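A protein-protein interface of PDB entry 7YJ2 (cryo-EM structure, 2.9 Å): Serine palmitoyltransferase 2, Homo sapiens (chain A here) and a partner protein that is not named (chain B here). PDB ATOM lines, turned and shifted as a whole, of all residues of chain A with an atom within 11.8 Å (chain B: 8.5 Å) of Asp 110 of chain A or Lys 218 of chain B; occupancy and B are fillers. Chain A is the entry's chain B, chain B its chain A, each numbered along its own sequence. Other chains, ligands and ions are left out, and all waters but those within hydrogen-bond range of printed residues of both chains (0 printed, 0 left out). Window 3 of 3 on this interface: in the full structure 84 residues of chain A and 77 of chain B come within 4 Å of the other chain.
Of the 22 printed residues of chain B, 7 touch a printed residue of chain A.
Printed residues of chain A that touch a printed residue of chain B: Arg 105, Gln 108, Asp 110, Phe 111, Val 112, Ser 113 and Leu 114.
Hydrophobic or aromatic side chains of chain A within 4 Å of the printed part of chain B: Phe 111, Val 112 and Leu 114.
Among the printed residues, 14 pairs touch across the chains.
Among the printed residues, no Asp or Glu carboxylate lies within 4 Å of a Lys or Arg side-chain nitrogen of the other chain.
Asp 110 of chain A touches just one residue of chain B: Lys 218.
Lys 218 of chain B touches just these residues of chain A: Asp 110 (3.6 Å) and Phe 111 (2.9 Å).
Printed residues of chain A within 4 Å of Arg 190 of chain B: Val 112 (3.8 Å).
Ala 219 of chain B touches none of the printed residues of chain A.
Printed residues of chain B within 4 Å of Val 112 of chain A: Thr 188 (3.5 Å), Arg 189 (3.9 Å), Arg 190 (3.8 Å) and Arg 220 (2.9 Å).
Of the printed residues of chain A, Thr 188 of chain B touches Val 112 (3.5 Å).
Printed residues of chain B within 4 Å of Leu 114 of chain A: Arg 189 (3.5 Å) and Arg 220 (3.8 Å).
Printed residues of chain B within 4 Å of Gln 108 of chain A: Lys 214 and Tyr 215.
Glu 104 of chain A touches none of the printed residues of chain B.
The nearest residue of chain B that does not touch Asp 110 of chain A is Tyr 215 of chain B (6.7 Å).
The nearest residue of chain A that does not touch Lys 218 of chain B is Val 112 of chain A (5.9 Å).
Among the printed residues, merely in contact across the chains: Phe 111 of chain A with Lys 218 of chain B (2.9 Å), Val 112 of chain A with Thr 188 of chain B (3.5 Å), Leu 114 of chain A with Arg 189 of chain B (3.5 Å), Asp 110 of chain A with Lys 218 of chain B (3.6 Å), Val 112 of chain A with Arg 190 of chain B (3.8 Å), Leu 114 of chain A with Arg 220 of chain B (3.8 Å), Val 112 of chain A with Arg 189 of chain B (3.9 Å), Gln 108 of chain A with Tyr 215 of chain B (3.9 Å), Phe 111 of chain A with Arg 220 of chain B (3.98 Å) and Phe 111 of chain A with Lys 214 of chain B (3.99 Å).
NH1 of Arg 105 of chain A sits close to NE2 of Gln 108 of chain A.
N of Ile 134 of chain B lies within hydrogen-bond range of O of Arg 189 of chain B (3.2 Å).
O of Ala 185 of chain B is in hydrogen-bond range of NH2 of Arg 190 of chain B (3.2 Å).
The guanidinium group (NH1) of Arg 190 of chain B lies within hydrogen-bond range of the backbone carbonyl oxygen (O) of Thr 188 of chain B, at 2.4 Å.
O of Arg 190 of chain B is in hydrogen-bond range of N of Arg 220 of chain B, 3.0 Å away.
The backbone carbonyl oxygen (O) of Arg 220 of chain B lies within hydrogen-bond range of the backbone NH (N) of Ile 192 of chain B (2.7 Å).
NH1 of Arg 105 of chain A lies within hydrogen-bond range of OH of Tyr 215 of chain B, 2.9 Å away.
The side-chain amino group of Lys 214 of chain B lies close to the side-chain amide nitrogen of Gln 108 of chain A, 3.1 Å away.
O of Val 112 of chain A is in hydrogen-bond range of NH2 of Arg 220 of chain B, 2.9 Å away.
NH2 of Arg 189 of chain B sits close to O of Ser 113 of chain A (2.4 Å).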
ATOM      1  N   THR A 103       7.599   8.658  22.725  1.00  0.00           N
ATOM      2  CA  THR A 103       7.069   8.951  21.402  1.00  0.00           C
ATOM      3  C   THR A 103       6.141   7.824  20.970  1.00  0.00           C
ATOM      4  O   THR A 103       5.937   6.845  21.688  1.00  0.00           O
ATOM      5  CB  THR A 103       8.186   9.138  20.371  1.00  0.00           C
ATOM      6  OG1 THR A 103       9.135   8.074  20.491  1.00  0.00           O
ATOM      7  CG2 THR A 103       8.887  10.458  20.569  1.00  0.00           C
ATOM      8  N   GLU A 104       5.580   7.984  19.777  1.00  0.00           N
ATOM      9  CA  GLU A 104       4.671   7.025  19.174  1.00  0.00           C
ATOM     10  C   GLU A 104       5.452   5.844  18.597  1.00  0.00           C
ATOM     11  O   GLU A 104       6.657   5.921  18.360  1.00  0.00           O
ATOM     12  CB  GLU A 104       3.855   7.731  18.091  1.00  0.00           C
ATOM     13  CG  GLU A 104       2.813   6.916  17.371  1.00  0.00           C
ATOM     14  CD  GLU A 104       1.697   6.473  18.268  1.00  0.00           C
ATOM     15  OE1 GLU A 104       1.450   7.152  19.275  1.00  0.00           O
ATOM     16  OE2 GLU A 104       1.051   5.457  17.968  1.00  0.00           O
ATOM     17  N   ARG A 105       4.754   4.734  18.379  1.00  0.00           N
ATOM     18  CA  ARG A 105       5.388   3.551  17.825  1.00  0.00           C
ATOM     19  C   ARG A 105       5.845   3.810  16.394  1.00  0.00           C
ATOM     20  O   ARG A 105       5.383   4.733  15.724  1.00  0.00           O
ATOM     21  CB  ARG A 105       4.437   2.358  17.845  1.00  0.00           C
ATOM     22  CG  ARG A 105       3.926   1.984  19.191  1.00  0.00           C
ATOM     23  CD  ARG A 105       2.836   0.933  19.116  1.00  0.00           C
ATOM     24  NE  ARG A 105       3.323  -0.378  18.710  1.00  0.00           N
ATOM     25  CZ  ARG A 105       2.846  -1.071  17.684  1.00  0.00           C
ATOM     26  NH1 ARG A 105       1.850  -0.592  16.966  1.00  0.00           N
ATOM     27  NH2 ARG A 105       3.348  -2.256  17.392  1.00  0.00           N
ATOM     28  N   GLU A 106       6.767   2.971  15.925  1.00  0.00           N
ATOM     29  CA  GLU A 106       7.189   3.034  14.533  1.00  0.00           C
ATOM     30  C   GLU A 106       6.082   2.623  13.580  1.00  0.00           C
ATOM     31  O   GLU A 106       6.051   3.097  12.442  1.00  0.00           O
ATOM     32  CB  GLU A 106       8.400   2.137  14.301  1.00  0.00           C
ATOM     33  CG  GLU A 106       9.709   2.696  14.799  1.00  0.00           C
ATOM     34  CD  GLU A 106      10.863   1.742  14.568  1.00  0.00           C
ATOM     35  OE1 GLU A 106      11.218   1.509  13.394  1.00  0.00           O
ATOM     36  OE2 GLU A 106      11.413   1.222  15.560  1.00  0.00           O
ATOM     37  N   GLU A 107       5.184   1.749  14.014  1.00  0.00           N
ATOM     38  CA  GLU A 107       4.126   1.246  13.156  1.00  0.00           C
ATOM     39  C   GLU A 107       2.963   2.211  13.019  1.00  0.00           C
ATOM     40  O   GLU A 107       2.147   2.049  12.110  1.00  0.00           O
ATOM     41  CB  GLU A 107       3.612  -0.087  13.692  1.00  0.00           C
ATOM     42  CG  GLU A 107       4.598  -1.241  13.594  1.00  0.00           C
ATOM     43  CD  GLU A 107       5.779  -1.098  14.526  1.00  0.00           C
ATOM     44  OE1 GLU A 107       6.782  -1.819  14.342  1.00  0.00           O
ATOM     45  OE2 GLU A 107       5.714  -0.252  15.436  1.00  0.00           O
ATOM     46  N   GLN A 108       2.870   3.211  13.883  1.00  0.00           N
ATOM     47  CA  GLN A 108       1.742   4.121  13.825  1.00  0.00           C
ATOM     48  C   GLN A 108       2.207   5.536  13.523  1.00  0.00           C
ATOM     49  O   GLN A 108       1.609   6.504  13.995  1.00  0.00           O
ATOM     50  CB  GLN A 108       0.972   4.073  15.138  1.00  0.00           C
ATOM     51  CG  GLN A 108       0.635   2.667  15.566  1.00  0.00           C
ATOM     52  CD  GLN A 108      -0.338   2.625  16.699  1.00  0.00           C
ATOM     53  OE1 GLN A 108      -0.820   3.653  17.153  1.00  0.00           O
ATOM     54  NE2 GLN A 108      -0.651   1.430  17.159  1.00  0.00           N
ATOM     55  N   LYS A 109       3.233   5.666  12.692  1.00  0.00           N
ATOM     56  CA  LYS A 109       3.738   6.981  12.331  1.00  0.00           C
ATOM     57  C   LYS A 109       2.811   7.703  11.356  1.00  0.00           C
ATOM     58  O   LYS A 109       2.847   8.925  11.257  1.00  0.00           O
ATOM     59  CB  LYS A 109       5.145   6.875  11.743  1.00  0.00           C
ATOM     60  CG  LYS A 109       5.485   5.508  11.182  1.00  0.00           C
ATOM     61  CD  LYS A 109       4.930   5.338   9.778  1.00  0.00           C
ATOM     62  CE  LYS A 109       4.567   3.890   9.500  1.00  0.00           C
ATOM     63  NZ  LYS A 109       5.745   3.102   9.052  1.00  0.00           N
ATOM     64  N   ASP A 110       1.979   6.950  10.640  1.00  0.00           N
ATOM     65  CA  ASP A 110       1.060   7.550   9.690  1.00  0.00           C
ATOM     66  C   ASP A 110      -0.387   7.562  10.161  1.00  0.00           C
ATOM     67  O   ASP A 110      -1.284   7.729   9.331  1.00  0.00           O
ATOM     68  CB  ASP A 110       1.174   6.849   8.335  1.00  0.00           C
ATOM     69  CG  ASP A 110       0.972   5.360   8.429  1.00  0.00           C
ATOM     70  OD1 ASP A 110       0.859   4.842   9.553  1.00  0.00           O
ATOM     71  OD2 ASP A 110       0.904   4.704   7.374  1.00  0.00           O
ATOM     72  N   PHE A 111      -0.646   7.391  11.453  1.00  0.00           N
ATOM     73  CA  PHE A 111      -1.964   7.729  11.959  1.00  0.00           C
ATOM     74  C   PHE A 111      -1.988   9.233  12.215  1.00  0.00           C
ATOM     75  O   PHE A 111      -0.944   9.882  12.263  1.00  0.00           O
ATOM     76  CB  PHE A 111      -2.298   7.009  13.268  1.00  0.00           C
ATOM     77  CG  PHE A 111      -2.398   5.521  13.156  1.00  0.00           C
ATOM     78  CD1 PHE A 111      -2.405   4.889  11.944  1.00  0.00           C
ATOM     79  CD2 PHE A 111      -2.663   4.771  14.275  1.00  0.00           C
ATOM     80  CE1 PHE A 111      -2.515   3.523  11.870  1.00  0.00           C
ATOM     81  CE2 PHE A 111      -2.805   3.418  14.195  1.00  0.00           C
ATOM     82  CZ  PHE A 111      -2.732   2.794  12.993  1.00  0.00           C
ATOM     83  N   VAL A 112      -3.183   9.790  12.396  1.00  0.00           N
ATOM     84  CA  VAL A 112      -3.267  11.169  12.857  1.00  0.00           C
ATOM     85  C   VAL A 112      -2.692  11.251  14.261  1.00  0.00           C
ATOM     86  O   VAL A 112      -2.882  10.347  15.079  1.00  0.00           O
ATOM     87  CB  VAL A 112      -4.719  11.667  12.815  1.00  0.00           C
ATOM     88  CG1 VAL A 112      -4.790  13.116  13.202  1.00  0.00           C
ATOM     89  CG2 VAL A 112      -5.290  11.474  11.443  1.00  0.00           C
ATOM     90  N   SER A 113      -1.972  12.329  14.546  1.00  0.00           N
ATOM     91  CA  SER A 113      -1.284  12.449  15.824  1.00  0.00           C
ATOM     92  C   SER A 113      -2.271  12.440  16.981  1.00  0.00           C
ATOM     93  O   SER A 113      -3.363  12.997  16.889  1.00  0.00           O
ATOM     94  CB  SER A 113      -0.462  13.731  15.853  1.00  0.00           C
ATOM     95  OG  SER A 113      -1.257  14.815  16.287  1.00  0.00           O
ATOM     96  N   LEU A 114      -1.872  11.803  18.083  1.00  0.00           N
ATOM     97  CA  LEU A 114      -2.783  11.615  19.204  1.00  0.00           C
ATOM     98  C   LEU A 114      -3.054  12.922  19.940  1.00  0.00           C
ATOM     99  O   LEU A 114      -4.200  13.210  20.298  1.00  0.00           O
ATOM    100  CB  LEU A 114      -2.228  10.550  20.149  1.00  0.00           C
ATOM    101  CG  LEU A 114      -3.040  10.169  21.383  1.00  0.00           C
ATOM    102  CD1 LEU A 114      -4.451   9.812  21.034  1.00  0.00           C
ATOM    103  CD2 LEU A 114      -2.390   9.007  22.058  1.00  0.00           C
ATOM    104  N   ILE B 134     -14.393  11.002  15.650  1.00  0.00           N
ATOM    105  CA  ILE B 134     -15.346   9.938  15.358  1.00  0.00           C
ATOM    106  C   ILE B 134     -15.008   8.727  16.209  1.00  0.00           C
ATOM    107  O   ILE B 134     -13.858   8.283  16.232  1.00  0.00           O
ATOM    108  CB  ILE B 134     -15.370   9.566  13.862  1.00  0.00           C
ATOM    109  CG1 ILE B 134     -15.868  10.729  13.017  1.00  0.00           C
ATOM    110  CG2 ILE B 134     -16.292   8.417  13.617  1.00  0.00           C
ATOM    111  CD1 ILE B 134     -14.840  11.644  12.548  1.00  0.00           C
ATOM    112  N   PHE B 136     -16.345   4.734  17.058  1.00  0.00           N
ATOM    113  CA  PHE B 136     -17.167   3.604  16.635  1.00  0.00           C
ATOM    114  C   PHE B 136     -17.335   2.675  17.832  1.00  0.00           C
ATOM    115  O   PHE B 136     -16.370   2.065  18.289  1.00  0.00           O
ATOM    116  CB  PHE B 136     -16.527   2.863  15.469  1.00  0.00           C
ATOM    117  CG  PHE B 136     -16.237   3.718  14.273  1.00  0.00           C
ATOM    118  CD1 PHE B 136     -17.115   3.768  13.213  1.00  0.00           C
ATOM    119  CD2 PHE B 136     -15.064   4.438  14.188  1.00  0.00           C
ATOM    120  CE1 PHE B 136     -16.839   4.538  12.114  1.00  0.00           C
ATOM    121  CE2 PHE B 136     -14.792   5.203  13.090  1.00  0.00           C
ATOM    122  CZ  PHE B 136     -15.680   5.252  12.054  1.00  0.00           C
ATOM    123  N   LEU B 171     -16.735   2.070   8.328  1.00  0.00           N
ATOM    124  CA  LEU B 171     -15.441   2.695   8.086  1.00  0.00           C
ATOM    125  C   LEU B 171     -15.256   3.119   6.634  1.00  0.00           C
ATOM    126  O   LEU B 171     -14.657   4.175   6.365  1.00  0.00           O
ATOM    127  CB  LEU B 171     -14.324   1.740   8.492  1.00  0.00           C
ATOM    128  CG  LEU B 171     -13.996   1.589   9.974  1.00  0.00           C
ATOM    129  CD1 LEU B 171     -13.046   0.449  10.163  1.00  0.00           C
ATOM    130  CD2 LEU B 171     -13.382   2.839  10.494  1.00  0.00           C
ATOM    131  N   GLU B 175     -14.336   6.878   4.743  1.00  0.00           N
ATOM    132  CA  GLU B 175     -13.246   7.058   3.792  1.00  0.00           C
ATOM    133  C   GLU B 175     -13.695   7.874   2.588  1.00  0.00           C
ATOM    134  O   GLU B 175     -12.899   8.570   1.972  1.00  0.00           O
ATOM    135  CB  GLU B 175     -12.723   5.704   3.329  1.00  0.00           C
ATOM    136  CG  GLU B 175     -11.213   5.601   3.303  1.00  0.00           C
ATOM    137  CD  GLU B 175     -10.743   4.250   2.811  1.00  0.00           C
ATOM    138  OE1 GLU B 175     -11.535   3.555   2.140  1.00  0.00           O
ATOM    139  OE2 GLU B 175      -9.585   3.880   3.095  1.00  0.00           O
ATOM    140  N   ASP B 178     -13.508  11.442   3.429  1.00  0.00           N
ATOM    141  CA  ASP B 178     -12.123  11.856   3.573  1.00  0.00           C
ATOM    142  C   ASP B 178     -11.597  12.306   2.218  1.00  0.00           C
ATOM    143  O   ASP B 178     -10.615  13.040   2.138  1.00  0.00           O
ATOM    144  CB  ASP B 178     -11.275  10.693   4.076  1.00  0.00           C
ATOM    145  CG  ASP B 178     -11.425  10.462   5.559  1.00  0.00           C
ATOM    146  OD1 ASP B 178     -10.686   9.620   6.106  1.00  0.00           O
ATOM    147  OD2 ASP B 178     -12.282  11.126   6.176  1.00  0.00           O
ATOM    148  N   ALA B 185      -9.714  15.921   7.238  1.00  0.00           N
ATOM    149  CA  ALA B 185      -9.458  14.540   7.604  1.00  0.00           C
ATOM    150  C   ALA B 185      -8.093  14.332   8.231  1.00  0.00           C
ATOM    151  O   ALA B 185      -7.836  13.254   8.768  1.00  0.00           O
ATOM    152  CB  ALA B 185      -9.591  13.639   6.380  1.00  0.00           C
ATOM    153  N   THR B 188      -8.537  14.903  12.320  1.00  0.00           N
ATOM    154  CA  THR B 188      -9.632  14.163  12.925  1.00  0.00           C
ATOM    155  C   THR B 188      -9.143  12.792  13.358  1.00  0.00           C
ATOM    156  O   THR B 188      -8.516  12.081  12.572  1.00  0.00           O
ATOM    157  CB  THR B 188     -10.787  14.013  11.941  1.00  0.00           C
ATOM    158  OG1 THR B 188     -11.397  15.287  11.721  1.00  0.00           O
ATOM    159  CG2 THR B 188     -11.812  13.103  12.500  1.00  0.00           C
ATOM    160  N   ARG B 189      -9.414  12.441  14.610  1.00  0.00           N
ATOM    161  CA  ARG B 189      -8.997  11.164  15.173  1.00  0.00           C
ATOM    162  C   ARG B 189     -10.120  10.135  15.138  1.00  0.00           C
ATOM    163  O   ARG B 189     -11.287  10.483  15.206  1.00  0.00           O
ATOM    164  CB  ARG B 189      -8.501  11.358  16.602  1.00  0.00           C
ATOM    165  CG  ARG B 189      -7.235  12.185  16.702  1.00  0.00           C
ATOM    166  CD  ARG B 189      -6.959  12.597  18.134  1.00  0.00           C
ATOM    167  NE  ARG B 189      -7.005  14.045  18.305  1.00  0.00           N
ATOM    168  CZ  ARG B 189      -6.196  14.898  17.688  1.00  0.00           C
ATOM    169  NH1 ARG B 189      -6.311  16.196  17.906  1.00  0.00           N
ATOM    170  NH2 ARG B 189      -5.271  14.453  16.853  1.00  0.00           N
ATOM    171  N   ARG B 190      -9.748   8.864  15.051  1.00  0.00           N
ATOM    172  CA  ARG B 190     -10.708   7.772  14.971  1.00  0.00           C
ATOM    173  C   ARG B 190     -10.412   6.740  16.047  1.00  0.00           C
ATOM    174  O   ARG B 190      -9.315   6.183  16.090  1.00  0.00           O
ATOM    175  CB  ARG B 190     -10.667   7.126  13.589  1.00  0.00           C
ATOM    176  CG  ARG B 190     -10.931   8.091  12.467  1.00  0.00           C
ATOM    177  CD  ARG B 190     -10.225   7.686  11.191  1.00  0.00           C
ATOM    178  NE  ARG B 190     -10.318   8.732  10.183  1.00  0.00           N
ATOM    179  CZ  ARG B 190      -9.630   9.866  10.223  1.00  0.00           C
ATOM    180  NH1 ARG B 190      -8.783  10.096  11.210  1.00  0.00           N
ATOM    181  NH2 ARG B 190      -9.787  10.771   9.271  1.00  0.00           N
ATOM    182  N   PHE B 191     -11.397   6.462  16.891  1.00  0.00           N
ATOM    183  CA  PHE B 191     -11.275   5.481  17.955  1.00  0.00           C
ATOM    184  C   PHE B 191     -12.335   4.408  17.788  1.00  0.00           C
ATOM    185  O   PHE B 191     -13.482   4.696  17.453  1.00  0.00           O
ATOM    186  CB  PHE B 191     -11.439   6.110  19.343  1.00  0.00           C
ATOM    187  CG  PHE B 191     -10.556   7.291  19.595  1.00  0.00           C
ATOM    188  CD1 PHE B 191      -9.312   7.125  20.152  1.00  0.00           C
ATOM    189  CD2 PHE B 191     -10.977   8.563  19.296  1.00  0.00           C
ATOM    190  CE1 PHE B 191      -8.505   8.196  20.388  1.00  0.00           C
ATOM    191  CE2 PHE B 191     -10.167   9.632  19.533  1.00  0.00           C
ATOM    192  CZ  PHE B 191      -8.934   9.448  20.079  1.00  0.00           C
ATOM    193  N   ILE B 192     -11.941   3.168  18.047  1.00  0.00           N
ATOM    194  CA  ILE B 192     -12.848   2.031  18.120  1.00  0.00           C
ATOM    195  C   ILE B 192     -12.892   1.594  19.574  1.00  0.00           C
ATOM    196  O   ILE B 192     -11.850   1.287  20.158  1.00  0.00           O
ATOM    197  CB  ILE B 192     -12.386   0.878  17.220  1.00  0.00           C
ATOM    198  CG1 ILE B 192     -12.216   1.353  15.783  1.00  0.00           C
ATOM    199  CG2 ILE B 192     -13.356  -0.267  17.298  1.00  0.00           C
ATOM    200  CD1 ILE B 192     -11.836   0.264  14.841  1.00  0.00           C
ATOM    201  N   VAL B 211      -8.151  -6.202  15.017  1.00  0.00           N
ATOM    202  CA  VAL B 211      -6.780  -5.717  14.899  1.00  0.00           C
ATOM    203  C   VAL B 211      -6.396  -5.440  13.458  1.00  0.00           C
ATOM    204  O   VAL B 211      -5.773  -4.412  13.186  1.00  0.00           O
ATOM    205  CB  VAL B 211      -5.789  -6.702  15.538  1.00  0.00           C
ATOM    206  CG1 VAL B 211      -4.384  -6.390  15.113  1.00  0.00           C
ATOM    207  CG2 VAL B 211      -5.879  -6.617  17.042  1.00  0.00           C
ATOM    208  N   LYS B 212      -6.814  -6.313  12.546  1.00  0.00           N
ATOM    209  CA  LYS B 212      -6.535  -6.144  11.124  1.00  0.00           C
ATOM    210  C   LYS B 212      -7.194  -4.877  10.593  1.00  0.00           C
ATOM    211  O   LYS B 212      -6.611  -4.165   9.789  1.00  0.00           O
ATOM    212  CB  LYS B 212      -6.993  -7.365  10.332  1.00  0.00           C
ATOM    213  CG  LYS B 212      -5.986  -8.501  10.330  1.00  0.00           C
ATOM    214  CD  LYS B 212      -6.416  -9.628   9.407  1.00  0.00           C
ATOM    215  CE  LYS B 212      -7.362 -10.590  10.108  1.00  0.00           C
ATOM    216  NZ  LYS B 212      -6.642 -11.677  10.825  1.00  0.00           N
ATOM    217  N   LEU B 213      -8.419  -4.605  11.024  1.00  0.00           N
ATOM    218  CA  LEU B 213      -9.094  -3.385  10.613  1.00  0.00           C
ATOM    219  C   LEU B 213      -8.409  -2.132  11.136  1.00  0.00           C
ATOM    220  O   LEU B 213      -8.499  -1.078  10.496  1.00  0.00           O
ATOM    221  CB  LEU B 213     -10.546  -3.405  11.083  1.00  0.00           C
ATOM    222  CG  LEU B 213     -11.499  -4.268  10.266  1.00  0.00           C
ATOM    223  CD1 LEU B 213     -12.866  -4.282  10.884  1.00  0.00           C
ATOM    224  CD2 LEU B 213     -11.579  -3.755   8.859  1.00  0.00           C
ATOM    225  N   LYS B 214      -7.724  -2.224  12.276  1.00  0.00           N
ATOM    226  CA  LYS B 214      -7.069  -1.061  12.864  1.00  0.00           C
ATOM    227  C   LYS B 214      -5.986  -0.506  11.957  1.00  0.00           C
ATOM    228  O   LYS B 214      -5.904   0.707  11.754  1.00  0.00           O
ATOM    229  CB  LYS B 214      -6.470  -1.426  14.220  1.00  0.00           C
ATOM    230  CG  LYS B 214      -5.627  -0.324  14.821  1.00  0.00           C
ATOM    231  CD  LYS B 214      -4.509  -0.816  15.691  1.00  0.00           C
ATOM    232  CE  LYS B 214      -4.179   0.238  16.708  1.00  0.00           C
ATOM    233  NZ  LYS B 214      -3.217  -0.240  17.707  1.00  0.00           N
ATOM    234  N   TYR B 215      -5.136  -1.373  11.422  1.00  0.00           N
ATOM    235  CA  TYR B 215      -4.041  -0.948  10.567  1.00  0.00           C
ATOM    236  C   TYR B 215      -4.469  -0.683   9.136  1.00  0.00           C
ATOM    237  O   TYR B 215      -3.730  -0.032   8.395  1.00  0.00           O
ATOM    238  CB  TYR B 215      -2.935  -2.000  10.591  1.00  0.00           C
ATOM    239  CG  TYR B 215      -2.182  -2.028  11.891  1.00  0.00           C
ATOM    240  CD1 TYR B 215      -1.377  -0.968  12.268  1.00  0.00           C
ATOM    241  CD2 TYR B 215      -2.280  -3.102  12.746  1.00  0.00           C
ATOM    242  CE1 TYR B 215      -0.691  -0.982  13.453  1.00  0.00           C
ATOM    243  CE2 TYR B 215      -1.597  -3.125  13.936  1.00  0.00           C
ATOM    244  CZ  TYR B 215      -0.805  -2.065  14.283  1.00  0.00           C
ATOM    245  OH  TYR B 215      -0.123  -2.093  15.471  1.00  0.00           O
ATOM    246  N   LYS B 216      -5.648  -1.149   8.738  1.00  0.00           N
ATOM    247  CA  LYS B 216      -6.157  -0.879   7.405  1.00  0.00           C
ATOM    248  C   LYS B 216      -6.919   0.430   7.317  1.00  0.00           C
ATOM    249  O   LYS B 216      -6.851   1.097   6.283  1.00  0.00           O
ATOM    250  CB  LYS B 216      -7.059  -2.017   6.946  1.00  0.00           C
ATOM    251  CG  LYS B 216      -7.473  -1.933   5.504  1.00  0.00           C
ATOM    252  CD  LYS B 216      -8.385  -3.081   5.161  1.00  0.00           C
ATOM    253  CE  LYS B 216      -8.906  -2.973   3.752  1.00  0.00           C
ATOM    254  NZ  LYS B 216      -9.929  -4.019   3.494  1.00  0.00           N
ATOM    255  N   TYR B 217      -7.632   0.824   8.367  1.00  0.00           N
ATOM    256  CA  TYR B 217      -8.365   2.078   8.337  1.00  0.00           C
ATOM    257  C   TYR B 217      -7.842   3.103   9.333  1.00  0.00           C
ATOM    258  O   TYR B 217      -8.397   4.202   9.417  1.00  0.00           O
ATOM    259  CB  TYR B 217      -9.852   1.819   8.565  1.00  0.00           C
ATOM    260  CG  TYR B 217     -10.494   1.170   7.374  1.00  0.00           C
ATOM    261  CD1 TYR B 217     -10.823   1.904   6.265  1.00  0.00           C
ATOM    262  CD2 TYR B 217     -10.744  -0.185   7.357  1.00  0.00           C
ATOM    263  CE1 TYR B 217     -11.390   1.312   5.182  1.00  0.00           C
ATOM    264  CE2 TYR B 217     -11.308  -0.783   6.278  1.00  0.00           C
ATOM    265  CZ  TYR B 217     -11.628  -0.031   5.193  1.00  0.00           C
ATOM    266  OH  TYR B 217     -12.195  -0.631   4.105  1.00  0.00           O
ATOM    267  N   LYS B 218      -6.727   2.790   9.978  1.00  0.00           N
ATOM    268  CA  LYS B 218      -6.064   3.706  10.898  1.00  0.00           C
ATOM    269  C   LYS B 218      -6.930   4.311  11.991  1.00  0.00           C
ATOM    270  O   LYS B 218      -7.163   5.514  12.026  1.00  0.00           O
ATOM    271  CB  LYS B 218      -5.368   4.814  10.113  1.00  0.00           C
ATOM    272  CG  LYS B 218      -4.018   4.398   9.561  1.00  0.00           C
ATOM    273  CD  LYS B 218      -3.673   5.181   8.310  1.00  0.00           C
ATOM    274  CE  LYS B 218      -2.886   4.330   7.333  1.00  0.00           C
ATOM    275  NZ  LYS B 218      -3.432   4.441   5.953  1.00  0.00           N
ATOM    276  N   ALA B 219      -7.378   3.453  12.892  1.00  0.00           N
ATOM    277  CA  ALA B 219      -8.190   3.835  14.033  1.00  0.00           C
ATOM    278  C   ALA B 219      -7.715   3.084  15.266  1.00  0.00           C
ATOM    279  O   ALA B 219      -7.584   1.864  15.230  1.00  0.00           O
ATOM    280  CB  ALA B 219      -9.662   3.541  13.770  1.00  0.00           C
ATOM    281  N   ARG B 220      -7.478   3.810  16.353  1.00  0.00           N
ATOM    282  CA  ARG B 220      -6.979   3.238  17.597  1.00  0.00           C
ATOM    283  C   ARG B 220      -8.061   2.444  18.318  1.00  0.00           C
ATOM    284  O   ARG B 220      -9.251   2.678  18.127  1.00  0.00           O
ATOM    285  CB  ARG B 220      -6.455   4.348  18.502  1.00  0.00           C
ATOM    286  CG  ARG B 220      -5.109   4.883  18.084  1.00  0.00           C
ATOM    287  CD  ARG B 220      -4.920   6.313  18.501  1.00  0.00           C
ATOM    288  NE  ARG B 220      -3.585   6.795  18.179  1.00  0.00           N
ATOM    289  CZ  ARG B 220      -3.327   7.761  17.307  1.00  0.00           C
ATOM    290  NH1 ARG B 220      -2.081   8.129  17.081  1.00  0.00           N
ATOM    291  NH2 ARG B 220      -4.310   8.361  16.663  1.00  0.00           N
ATOM    292  N   ILE B 221      -7.640   1.507  19.164  1.00  0.00           N
ATOM    293  CA  ILE B 221      -8.541   0.604  19.877  1.00  0.00           C
ATOM    294  C   ILE B 221      -8.510   0.937  21.363  1.00  0.00           C
ATOM    295  O   ILE B 221      -7.462   1.284  21.902  1.00  0.00           O
ATOM    296  CB  ILE B 221      -8.166  -0.869  19.644  1.00  0.00           C
ATOM    297  CG1 ILE B 221      -8.183  -1.201  18.158  1.00  0.00           C
ATOM    298  CG2 ILE B 221      -9.108  -1.788  20.371  1.00  0.00           C
ATOM    299  CD1 ILE B 221      -7.743  -2.603  17.853  1.00  0.00           C
